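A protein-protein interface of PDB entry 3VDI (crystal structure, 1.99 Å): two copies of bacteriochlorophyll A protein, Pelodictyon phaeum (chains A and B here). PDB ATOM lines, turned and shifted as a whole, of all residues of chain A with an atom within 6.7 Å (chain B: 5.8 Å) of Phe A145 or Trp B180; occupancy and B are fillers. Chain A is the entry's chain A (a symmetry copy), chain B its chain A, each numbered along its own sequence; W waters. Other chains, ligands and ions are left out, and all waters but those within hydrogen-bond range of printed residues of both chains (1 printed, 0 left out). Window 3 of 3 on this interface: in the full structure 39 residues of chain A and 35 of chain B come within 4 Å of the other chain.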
ATOM      1  N   SER A 118       0.289 -26.499 -36.175  1.00  0.00           N
ATOM      2  CA  SER A 118      -0.605 -26.970 -35.127  1.00  0.00           C
ATOM      3  C   SER A 118      -0.799 -25.796 -34.183  1.00  0.00           C
ATOM      4  O   SER A 118       0.137 -25.040 -33.926  1.00  0.00           O
ATOM      5  CB  SER A 118      -0.042 -28.188 -34.402  1.00  0.00           C
ATOM      6  OG  SER A 118       0.960 -27.823 -33.469  1.00  0.00           O
ATOM      7  N   VAL A 119      -2.027 -25.607 -33.712  1.00  0.00           N
ATOM      8  CA  VAL A 119      -2.364 -24.521 -32.797  1.00  0.00           C
ATOM      9  C   VAL A 119      -3.081 -25.163 -31.633  1.00  0.00           C
ATOM     10  O   VAL A 119      -4.101 -25.808 -31.845  1.00  0.00           O
ATOM     11  CB  VAL A 119      -3.208 -23.387 -33.445  1.00  0.00           C
ATOM     12  CG1 VAL A 119      -3.540 -22.308 -32.402  1.00  0.00           C
ATOM     13  CG2 VAL A 119      -2.479 -22.758 -34.638  1.00  0.00           C
ATOM     14  N   VAL A 120      -2.549 -24.998 -30.421  1.00  0.00           N
ATOM     15  CA  VAL A 120      -3.106 -25.593 -29.208  1.00  0.00           C
ATOM     16  C   VAL A 120      -3.629 -24.482 -28.308  1.00  0.00           C
ATOM     17  O   VAL A 120      -2.849 -23.641 -27.842  1.00  0.00           O
ATOM     18  CB  VAL A 120      -2.085 -26.520 -28.469  1.00  0.00           C
ATOM     19  CG1 VAL A 120      -2.700 -27.136 -27.205  1.00  0.00           C
ATOM     20  CG2 VAL A 120      -1.556 -27.628 -29.391  1.00  0.00           C
ATOM     21  N   ASN A 121      -4.934 -24.471 -28.066  1.00  0.00           N
ATOM     22  CA  ASN A 121      -5.513 -23.474 -27.174  1.00  0.00           C
ATOM     23  C   ASN A 121      -5.503 -23.984 -25.725  1.00  0.00           C
ATOM     24  O   ASN A 121      -5.841 -25.139 -25.484  1.00  0.00           O
ATOM     25  CB  ASN A 121      -6.940 -23.114 -27.607  1.00  0.00           C
ATOM     26  CG  ASN A 121      -7.421 -21.851 -26.949  1.00  0.00           C
ATOM     27  OD1 ASN A 121      -6.854 -20.780 -27.133  1.00  0.00           O
ATOM     28  ND2 ASN A 121      -8.470 -21.944 -26.163  1.00  0.00           N
ATOM     29  N   MET A 122      -5.097 -23.141 -24.770  1.00  0.00           N
ATOM     30  CA  MET A 122      -5.063 -23.546 -23.357  1.00  0.00           C
ATOM     31  C   MET A 122      -5.742 -22.481 -22.490  1.00  0.00           C
ATOM     32  O   MET A 122      -5.138 -21.450 -22.165  1.00  0.00           O
ATOM     33  CB  MET A 122      -3.619 -23.802 -22.871  1.00  0.00           C
ATOM     34  CG  MET A 122      -3.510 -24.232 -21.393  1.00  0.00           C
ATOM     35  SD  MET A 122      -1.781 -24.327 -20.817  1.00  0.00           S
ATOM     36  CE  MET A 122      -1.438 -22.634 -20.595  1.00  0.00           C
ATOM     37  N   TYR A 124      -6.810 -20.879 -19.138  1.00  0.00           N
ATOM     38  CA  TYR A 124      -6.088 -20.887 -17.858  1.00  0.00           C
ATOM     39  C   TYR A 124      -6.786 -21.641 -16.710  1.00  0.00           C
ATOM     40  O   TYR A 124      -6.127 -22.084 -15.758  1.00  0.00           O
ATOM     41  CB  TYR A 124      -5.685 -19.470 -17.450  1.00  0.00           C
ATOM     42  CG  TYR A 124      -4.465 -18.944 -18.176  1.00  0.00           C
ATOM     43  CD1 TYR A 124      -3.476 -19.805 -18.648  1.00  0.00           C
ATOM     44  CD2 TYR A 124      -4.273 -17.576 -18.349  1.00  0.00           C
ATOM     45  CE1 TYR A 124      -2.327 -19.314 -19.280  1.00  0.00           C
ATOM     46  CE2 TYR A 124      -3.133 -17.079 -18.986  1.00  0.00           C
ATOM     47  CZ  TYR A 124      -2.157 -17.949 -19.438  1.00  0.00           C
ATOM     48  OH  TYR A 124      -1.054 -17.439 -20.075  1.00  0.00           O
ATOM     49  N   ARG A 143      -3.775 -19.050 -23.029  1.00  0.00           N
ATOM     50  CA  ARG A 143      -2.581 -18.929 -23.850  1.00  0.00           C
ATOM     51  C   ARG A 143      -2.725 -19.939 -24.999  1.00  0.00           C
ATOM     52  O   ARG A 143      -3.308 -21.009 -24.825  1.00  0.00           O
ATOM     53  CB  ARG A 143      -1.309 -19.169 -22.992  1.00  0.00           C
ATOM     54  CG  ARG A 143       0.014 -18.975 -23.747  1.00  0.00           C
ATOM     55  CD  ARG A 143       1.219 -18.882 -22.792  1.00  0.00           C
ATOM     56  NE  ARG A 143       1.279 -17.565 -22.126  1.00  0.00           N
ATOM     57  CZ  ARG A 143       1.962 -16.514 -22.570  1.00  0.00           C
ATOM     58  NH1 ARG A 143       2.703 -16.608 -23.667  1.00  0.00           N
ATOM     59  NH2 ARG A 143       1.942 -15.371 -21.900  1.00  0.00           N
ATOM     60  N   GLN A 144      -2.203 -19.579 -26.170  1.00  0.00           N
ATOM     61  CA  GLN A 144      -2.346 -20.372 -27.378  1.00  0.00           C
ATOM     62  C   GLN A 144      -1.003 -20.529 -28.090  1.00  0.00           C
ATOM     63  O   GLN A 144      -0.373 -19.554 -28.476  1.00  0.00           O
ATOM     64  CB  GLN A 144      -3.381 -19.690 -28.275  1.00  0.00           C
ATOM     65  CG  GLN A 144      -3.801 -20.523 -29.452  1.00  0.00           C
ATOM     66  CD  GLN A 144      -4.821 -19.740 -30.225  1.00  0.00           C
ATOM     67  OE1 GLN A 144      -4.490 -18.996 -31.148  1.00  0.00           O
ATOM     68  NE2 GLN A 144      -6.064 -19.816 -29.793  1.00  0.00           N
ATOM     69  N   PHE A 145      -0.635 -21.766 -28.310  1.00  0.00           N
ATOM     70  CA  PHE A 145       0.654 -22.245 -28.806  1.00  0.00           C
ATOM     71  C   PHE A 145       0.631 -22.590 -30.289  1.00  0.00           C
ATOM     72  O   PHE A 145      -0.142 -23.450 -30.712  1.00  0.00           O
ATOM     73  CB  PHE A 145       1.085 -23.473 -27.958  1.00  0.00           C
ATOM     74  CG  PHE A 145       1.150 -23.175 -26.470  1.00  0.00           C
ATOM     75  CD1 PHE A 145       2.345 -22.765 -25.874  1.00  0.00           C
ATOM     76  CD2 PHE A 145       0.016 -23.285 -25.666  1.00  0.00           C
ATOM     77  CE1 PHE A 145       2.399 -22.458 -24.510  1.00  0.00           C
ATOM     78  CE2 PHE A 145       0.069 -22.954 -24.311  1.00  0.00           C
ATOM     79  CZ  PHE A 145       1.266 -22.549 -23.741  1.00  0.00           C
ATOM     80  N   HIS A 146       1.500 -21.934 -31.058  1.00  0.00           N
ATOM     81  CA  HIS A 146       1.668 -22.177 -32.493  1.00  0.00           C
ATOM     82  C   HIS A 146       2.986 -22.938 -32.715  1.00  0.00           C
ATOM     83  O   HIS A 146       3.997 -22.635 -32.088  1.00  0.00           O
ATOM     84  CB  HIS A 146       1.712 -20.870 -33.297  1.00  0.00           C
ATOM     85  CG  HIS A 146       0.376 -20.221 -33.582  1.00  0.00           C
ATOM     86  ND1 HIS A 146      -0.467 -19.810 -32.567  1.00  0.00           N
ATOM     87  CD2 HIS A 146      -0.172 -19.870 -34.771  1.00  0.00           C
ATOM     88  CE1 HIS A 146      -1.518 -19.267 -33.168  1.00  0.00           C
ATOM     89  NE2 HIS A 146      -1.384 -19.278 -34.491  1.00  0.00           N
ATOM     90  N   ASP A 147       2.956 -23.901 -33.613  1.00  0.00           N
ATOM     91  CA  ASP A 147       4.099 -24.712 -34.037  1.00  0.00           C
ATOM     92  C   ASP A 147       3.944 -24.725 -35.558  1.00  0.00           C
ATOM     93  O   ASP A 147       3.074 -25.419 -36.079  1.00  0.00           O
ATOM     94  CB  ASP A 147       4.006 -26.153 -33.467  1.00  0.00           C
ATOM     95  CG  ASP A 147       5.157 -27.086 -33.861  1.00  0.00           C
ATOM     96  OD1 ASP A 147       6.051 -26.646 -34.608  1.00  0.00           O
ATOM     97  OD2 ASP A 147       5.209 -28.215 -33.339  1.00  0.00           O
ATOM     98  N   ARG A 200      -0.607 -10.762 -25.340  1.00  0.00           N
ATOM     99  CA  ARG A 200       0.844 -10.914 -25.194  1.00  0.00           C
ATOM    100  C   ARG A 200       1.372 -11.786 -26.336  1.00  0.00           C
ATOM    101  O   ARG A 200       0.711 -12.743 -26.714  1.00  0.00           O
ATOM    102  CB  ARG A 200       1.161 -11.609 -23.856  1.00  0.00           C
ATOM    103  CG  ARG A 200       0.798 -10.788 -22.627  1.00  0.00           C
ATOM    104  CD  ARG A 200       1.240 -11.474 -21.349  1.00  0.00           C
ATOM    105  NE  ARG A 200       2.703 -11.450 -21.182  1.00  0.00           N
ATOM    106  CZ  ARG A 200       3.368 -12.132 -20.252  1.00  0.00           C
ATOM    107  NH1 ARG A 200       2.720 -12.944 -19.422  1.00  0.00           N
ATOM    108  NH2 ARG A 200       4.688 -12.057 -20.184  1.00  0.00           N
ATOM    109  N   SER A 202       4.777 -14.069 -27.158  1.00  0.00           N
ATOM    110  CA  SER A 202       6.014 -14.631 -26.624  1.00  0.00           C
ATOM    111  C   SER A 202       7.157 -14.453 -27.635  1.00  0.00           C
ATOM    112  O   SER A 202       6.892 -14.315 -28.833  1.00  0.00           O
ATOM    113  CB  SER A 202       5.836 -16.132 -26.354  1.00  0.00           C
ATOM    114  OG  SER A 202       6.114 -16.918 -27.511  1.00  0.00           O
ATOM    115  N   PHE A 226       5.712 -20.081 -31.175  1.00  0.00           N
ATOM    116  CA  PHE A 226       5.445 -18.922 -30.337  1.00  0.00           C
ATOM    117  C   PHE A 226       4.121 -19.199 -29.647  1.00  0.00           C
ATOM    118  O   PHE A 226       3.370 -20.069 -30.090  1.00  0.00           O
ATOM    119  CB  PHE A 226       5.364 -17.606 -31.181  1.00  0.00           C
ATOM    120  CG  PHE A 226       4.065 -17.372 -31.932  1.00  0.00           C
ATOM    121  CD1 PHE A 226       3.035 -16.626 -31.361  1.00  0.00           C
ATOM    122  CD2 PHE A 226       3.896 -17.844 -33.231  1.00  0.00           C
ATOM    123  CE1 PHE A 226       1.849 -16.389 -32.059  1.00  0.00           C
ATOM    124  CE2 PHE A 226       2.712 -17.589 -33.941  1.00  0.00           C
ATOM    125  CZ  PHE A 226       1.702 -16.856 -33.355  1.00  0.00           C
ATOM    126  N   SER A 227       3.843 -18.473 -28.573  1.00  0.00           N
ATOM    127  CA  SER A 227       2.545 -18.534 -27.929  1.00  0.00           C
ATOM    128  C   SER A 227       2.033 -17.112 -27.842  1.00  0.00           C
ATOM    129  O   SER A 227       2.818 -16.168 -27.813  1.00  0.00           O
ATOM    130  CB  SER A 227       2.611 -19.159 -26.535  1.00  0.00           C
ATOM    131  OG  SER A 227       3.394 -18.439 -25.600  1.00  0.00           O
ATOM    132  N   HIS A 228       0.728 -16.961 -27.828  1.00  0.00           N
ATOM    133  CA  HIS A 228       0.131 -15.662 -27.582  1.00  0.00           C
ATOM    134  C   HIS A 228      -0.869 -15.904 -26.469  1.00  0.00           C
ATOM    135  O   HIS A 228      -1.305 -17.036 -26.280  1.00  0.00           O
ATOM    136  CB  HIS A 228      -0.434 -14.978 -28.846  1.00  0.00           C
ATOM    137  CG  HIS A 228      -1.710 -15.569 -29.366  1.00  0.00           C
ATOM    138  ND1 HIS A 228      -2.896 -14.876 -29.293  1.00  0.00           N
ATOM    139  CD2 HIS A 228      -1.935 -16.768 -29.955  1.00  0.00           C
ATOM    140  CE1 HIS A 228      -3.803 -15.660 -29.858  1.00  0.00           C
ATOM    141  NE2 HIS A 228      -3.279 -16.823 -30.236  1.00  0.00           N
ATOM    142  N   ALA A 229      -1.110 -14.895 -25.646  1.00  0.00           N
ATOM    143  CA  ALA A 229      -2.003 -15.041 -24.504  1.00  0.00           C
ATOM    144  C   ALA A 229      -2.959 -13.870 -24.458  1.00  0.00           C
ATOM    145  O   ALA A 229      -2.726 -12.858 -25.108  1.00  0.00           O
ATOM    146  CB  ALA A 229      -1.198 -15.114 -23.210  1.00  0.00           C
ATOM    147  N   VAL B 175       8.783 -21.794 -14.079  1.00  0.00           N
ATOM    148  CA  VAL B 175       9.075 -20.358 -14.242  1.00  0.00           C
ATOM    149  C   VAL B 175       7.946 -19.652 -15.008  1.00  0.00           C
ATOM    150  O   VAL B 175       7.749 -18.441 -14.856  1.00  0.00           O
ATOM    151  CB  VAL B 175      10.489 -20.179 -14.888  1.00  0.00           C
ATOM    152  CG1 VAL B 175      10.649 -18.850 -15.610  1.00  0.00           C
ATOM    153  CG2 VAL B 175      11.588 -20.356 -13.846  1.00  0.00           C
ATOM    154  N   ASN B 176       7.184 -20.407 -15.806  1.00  0.00           N
ATOM    155  CA  ASN B 176       6.099 -19.816 -16.569  1.00  0.00           C
ATOM    156  C   ASN B 176       4.899 -19.447 -15.712  1.00  0.00           C
ATOM    157  O   ASN B 176       4.190 -18.513 -16.081  1.00  0.00           O
ATOM    158  CB  ASN B 176       5.669 -20.716 -17.738  1.00  0.00           C
ATOM    159  CG  ASN B 176       6.752 -20.946 -18.760  1.00  0.00           C
ATOM    160  OD1 ASN B 176       7.540 -20.052 -19.109  1.00  0.00           O
ATOM    161  ND2 ASN B 176       6.800 -22.156 -19.260  1.00  0.00           N
ATOM    162  N   PHE B 177       4.672 -20.153 -14.579  1.00  0.00           N
ATOM    163  CA  PHE B 177       3.514 -19.861 -13.725  1.00  0.00           C
ATOM    164  C   PHE B 177       3.457 -18.388 -13.273  1.00  0.00           C
ATOM    165  O   PHE B 177       2.444 -17.731 -13.485  1.00  0.00           O
ATOM    166  CB  PHE B 177       3.399 -20.815 -12.511  1.00  0.00           C
ATOM    167  CG  PHE B 177       2.267 -20.375 -11.597  1.00  0.00           C
ATOM    168  CD1 PHE B 177       0.947 -20.693 -11.898  1.00  0.00           C
ATOM    169  CD2 PHE B 177       2.514 -19.548 -10.502  1.00  0.00           C
ATOM    170  CE1 PHE B 177      -0.098 -20.250 -11.085  1.00  0.00           C
ATOM    171  CE2 PHE B 177       1.467 -19.076  -9.713  1.00  0.00           C
ATOM    172  CZ  PHE B 177       0.172 -19.458  -9.986  1.00  0.00           C
ATOM    173  N   GLY B 178       4.532 -17.912 -12.641  1.00  0.00           N
ATOM    174  CA  GLY B 178       4.607 -16.550 -12.126  1.00  0.00           C
ATOM    175  C   GLY B 178       4.530 -15.484 -13.206  1.00  0.00           C
ATOM    176  O   GLY B 178       4.103 -14.363 -12.939  1.00  0.00           O
ATOM    177  N   ASP B 179       4.948 -15.833 -14.426  1.00  0.00           N
ATOM    178  CA  ASP B 179       4.910 -14.954 -15.579  1.00  0.00           C
ATOM    179  C   ASP B 179       3.462 -14.883 -16.158  1.00  0.00           C
ATOM    180  O   ASP B 179       2.862 -13.805 -16.188  1.00  0.00           O
ATOM    181  CB  ASP B 179       5.938 -15.458 -16.629  1.00  0.00           C
ATOM    182  CG  ASP B 179       5.928 -14.739 -17.975  1.00  0.00           C
ATOM    183  OD1 ASP B 179       5.267 -13.678 -18.082  1.00  0.00           O
ATOM    184  OD2 ASP B 179       6.530 -15.268 -18.932  1.00  0.00           O
ATOM    185  N   TRP B 180       2.906 -16.038 -16.575  1.00  0.00           N
ATOM    186  CA  TRP B 180       1.601 -16.132 -17.243  1.00  0.00           C
ATOM    187  C   TRP B 180       0.407 -15.848 -16.346  1.00  0.00           C
ATOM    188  O   TRP B 180      -0.667 -15.567 -16.858  1.00  0.00           O
ATOM    189  CB  TRP B 180       1.439 -17.500 -17.939  1.00  0.00           C
ATOM    190  CG  TRP B 180       2.490 -17.853 -18.963  1.00  0.00           C
ATOM    191  CD1 TRP B 180       3.449 -17.034 -19.489  1.00  0.00           C
ATOM    192  CD2 TRP B 180       2.681 -19.138 -19.572  1.00  0.00           C
ATOM    193  NE1 TRP B 180       4.242 -17.738 -20.368  1.00  0.00           N
ATOM    194  CE2 TRP B 180       3.800 -19.035 -20.432  1.00  0.00           C
ATOM    195  CE3 TRP B 180       2.027 -20.378 -19.460  1.00  0.00           C
ATOM    196  CZ2 TRP B 180       4.257 -20.119 -21.206  1.00  0.00           C
ATOM    197  CZ3 TRP B 180       2.488 -21.452 -20.218  1.00  0.00           C
ATOM    198  CH2 TRP B 180       3.598 -21.319 -21.069  1.00  0.00           C
ATOM    199  N   ILE B 181       0.577 -15.933 -15.003  1.00  0.00           N
ATOM    200  CA  ILE B 181      -0.523 -15.654 -14.076  1.00  0.00           C
ATOM    201  C   ILE B 181      -1.012 -14.211 -14.203  1.00  0.00           C
ATOM    202  O   ILE B 181      -2.147 -13.937 -13.832  1.00  0.00           O
ATOM    203  CB  ILE B 181      -0.151 -16.009 -12.592  1.00  0.00           C
ATOM    204  CG1 ILE B 181      -1.400 -16.120 -11.680  1.00  0.00           C
ATOM    205  CG2 ILE B 181       0.898 -15.049 -12.020  1.00  0.00           C
ATOM    206  CD1 ILE B 181      -2.338 -17.298 -12.070  1.00  0.00           C
ATOM    207  N   ARG B 182      -0.151 -13.288 -14.666  1.00  0.00           N
ATOM    208  CA  ARG B 182      -0.509 -11.859 -14.778  1.00  0.00           C
ATOM    209  C   ARG B 182      -1.716 -11.596 -15.655  1.00  0.00           C
ATOM    210  O   ARG B 182      -2.574 -10.811 -15.252  1.00  0.00           O
ATOM    211  CB  ARG B 182       0.702 -10.992 -15.150  1.00  0.00           C
ATOM    212  CG  ARG B 182       1.732 -10.936 -13.987  1.00  0.00           C
ATOM    213  CD  ARG B 182       2.993 -10.199 -14.346  1.00  0.00           C
ATOM    214  NE  ARG B 182       3.819 -10.987 -15.266  1.00  0.00           N
ATOM    215  CZ  ARG B 182       4.988 -10.590 -15.746  1.00  0.00           C
ATOM    216  NH1 ARG B 182       5.502  -9.417 -15.385  1.00  0.00           N
ATOM    217  NH2 ARG B 182       5.656 -11.359 -16.594  1.00  0.00           N
ATOM    218  N   GLU B 183      -1.850 -12.323 -16.785  1.00  0.00           N
ATOM    219  CA  GLU B 183      -3.006 -12.132 -17.676  1.00  0.00           C
ATOM    220  C   GLU B 183      -4.260 -12.830 -17.151  1.00  0.00           C
ATOM    221  O   GLU B 183      -5.335 -12.536 -17.608  1.00  0.00           O
ATOM    222  CB  GLU B 183      -2.706 -12.499 -19.144  1.00  0.00           C
ATOM    223  CG  GLU B 183      -2.177 -13.915 -19.357  1.00  0.00           C
ATOM    224  CD  GLU B 183      -0.668 -14.072 -19.403  1.00  0.00           C
ATOM    225  OE1 GLU B 183      -0.199 -15.082 -19.970  1.00  0.00           O
ATOM    226  OE2 GLU B 183       0.045 -13.236 -18.805  1.00  0.00           O
ATOM    227  N   PHE B 184      -4.117 -13.790 -16.227  1.00  0.00           N
ATOM    228  CA  PHE B 184      -5.253 -14.443 -15.584  1.00  0.00           C
ATOM    229  C   PHE B 184      -5.803 -13.452 -14.530  1.00  0.00           C
ATOM    230  O   PHE B 184      -7.013 -13.247 -14.398  1.00  0.00           O
ATOM    231  CB  PHE B 184      -4.778 -15.744 -14.885  1.00  0.00           C
ATOM    232  CG  PHE B 184      -5.767 -16.298 -13.886  1.00  0.00           C
ATOM    233  CD1 PHE B 184      -6.811 -17.124 -14.299  1.00  0.00           C
ATOM    234  CD2 PHE B 184      -5.668 -15.981 -12.533  1.00  0.00           C
ATOM    235  CE1 PHE B 184      -7.721 -17.649 -13.367  1.00  0.00           C
ATOM    236  CE2 PHE B 184      -6.577 -16.504 -11.602  1.00  0.00           C
ATOM    237  CZ  PHE B 184      -7.600 -17.331 -12.030  1.00  0.00           C
HETATM  238  O   HOH W   1       7.944 -12.481 -19.986  1.00  0.00           O
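The guanidinium group of Arg A200 lies within salt-bridge range of the side-chain carboxylate of Asp B179 (2.7 Å). OH of Tyr A124 is in hydrogen-bond range of OE1 of Glu B183, at 2.5 Å. The guanidinium group of Arg A143 is in salt-bridge range of the side-chain carboxylate of Glu B183, at 2.9 Å. OE2 of Glu B183 is in salt-bridge range of NH1 of Arg A200 (2.8 Å). The guanidinium group (NE) of Arg A143 lies close to the indole nitrogen (NE1) of Trp B180 (3.4 Å).
NH2 of Arg B182 lies within salt-bridge range of OD1 of Asp B179 (2.8 Å). The backbone NH of Val A120 sits at hydrogen-bond distance from the backbone carbonyl oxygen of Phe A145, at 2.9 Å. The backbone carbonyl oxygen of Arg A143 lies within hydrogen-bond range of the backbone NH of Met A122, at 2.8 Å. The guanidinium group (NE) of Arg A143 lies within hydrogen-bond range of the side-chain hydroxyl (OH) of Tyr A124 (3.1 Å). OG of Ser A227 sits at hydrogen-bond distance from NH1 of Arg A143 (2.8 Å). O of Ala A229 sits at hydrogen-bond distance from N of Arg A200, at 3.0 Å.
Tyr A124 touches Trp B180 (OH to CB, 3.3 Å). CD2 of Tyr A124 touches CB of Phe B184, at 3.95 Å. CZ of Phe A145 touches CH2 of Trp B180, 3.8 Å away. Arg B182 touches Arg A200 (NH2 to NH2, 3.8 Å). OE1 of Glu B183 touches CB of Ala A229 (3.4 Å).
Phe A145 touches one residue of chain B. Of chain A, only Tyr A124, Arg A143 and Phe A145 come within 4 Å of Trp B180. Printed residues of chain A within 4 Å of Glu B183: Tyr A124, Arg A143, Arg A200 and Ala A229. Printed residues of chain A within 4 Å of Phe B184: Tyr A124. Printed residues of chain B within 4 Å of Ala A229: Glu B183 (3.4 Å). Printed residues of chain B within 4 Å of Arg A143: Trp B180 and Glu B183. Ile B181 touches none of the printed residues of chain A. The nearest printed residue of chain B that does not touch Phe A145 is Asn B176 (6.9 Å). The nearest printed residue of chain B that does not touch Arg A200 is Trp B180 (4.02 Å).
Hydrophobic or aromatic side chains of chain B that line the printed part of chain A: Trp B180 and Phe B184. Of the 17 printed residues of chain A, 5 touch a printed residue of chain B. Hydrophobic or aromatic side chains of chain A that line the printed part of chain B: Tyr A124, Phe A145 and Ala A229. Along chain A the printed residues that touch a printed residue of chain B span positions 124 to 229. Among the printed residues, Asp or Glu carboxylates within 4 Å of a Lys or Arg side-chain nitrogen of the other chain: Arg A143 with Glu B183 (2.9 Å), Arg A200 with Asp B179 (2.7 Å) and Arg A200 with Glu B183 (2.8 Å).
No position is printed for both chains. Of the 10 pairs that touch across the chains among the printed residues, none has its exchanged pair printed and touching as well.
Water W1 lies within hydrogen-bond range of the guanidinium group of Arg A200 (3.3 Å) and the side-chain carboxylate of Asp B179 (3.3 Å).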
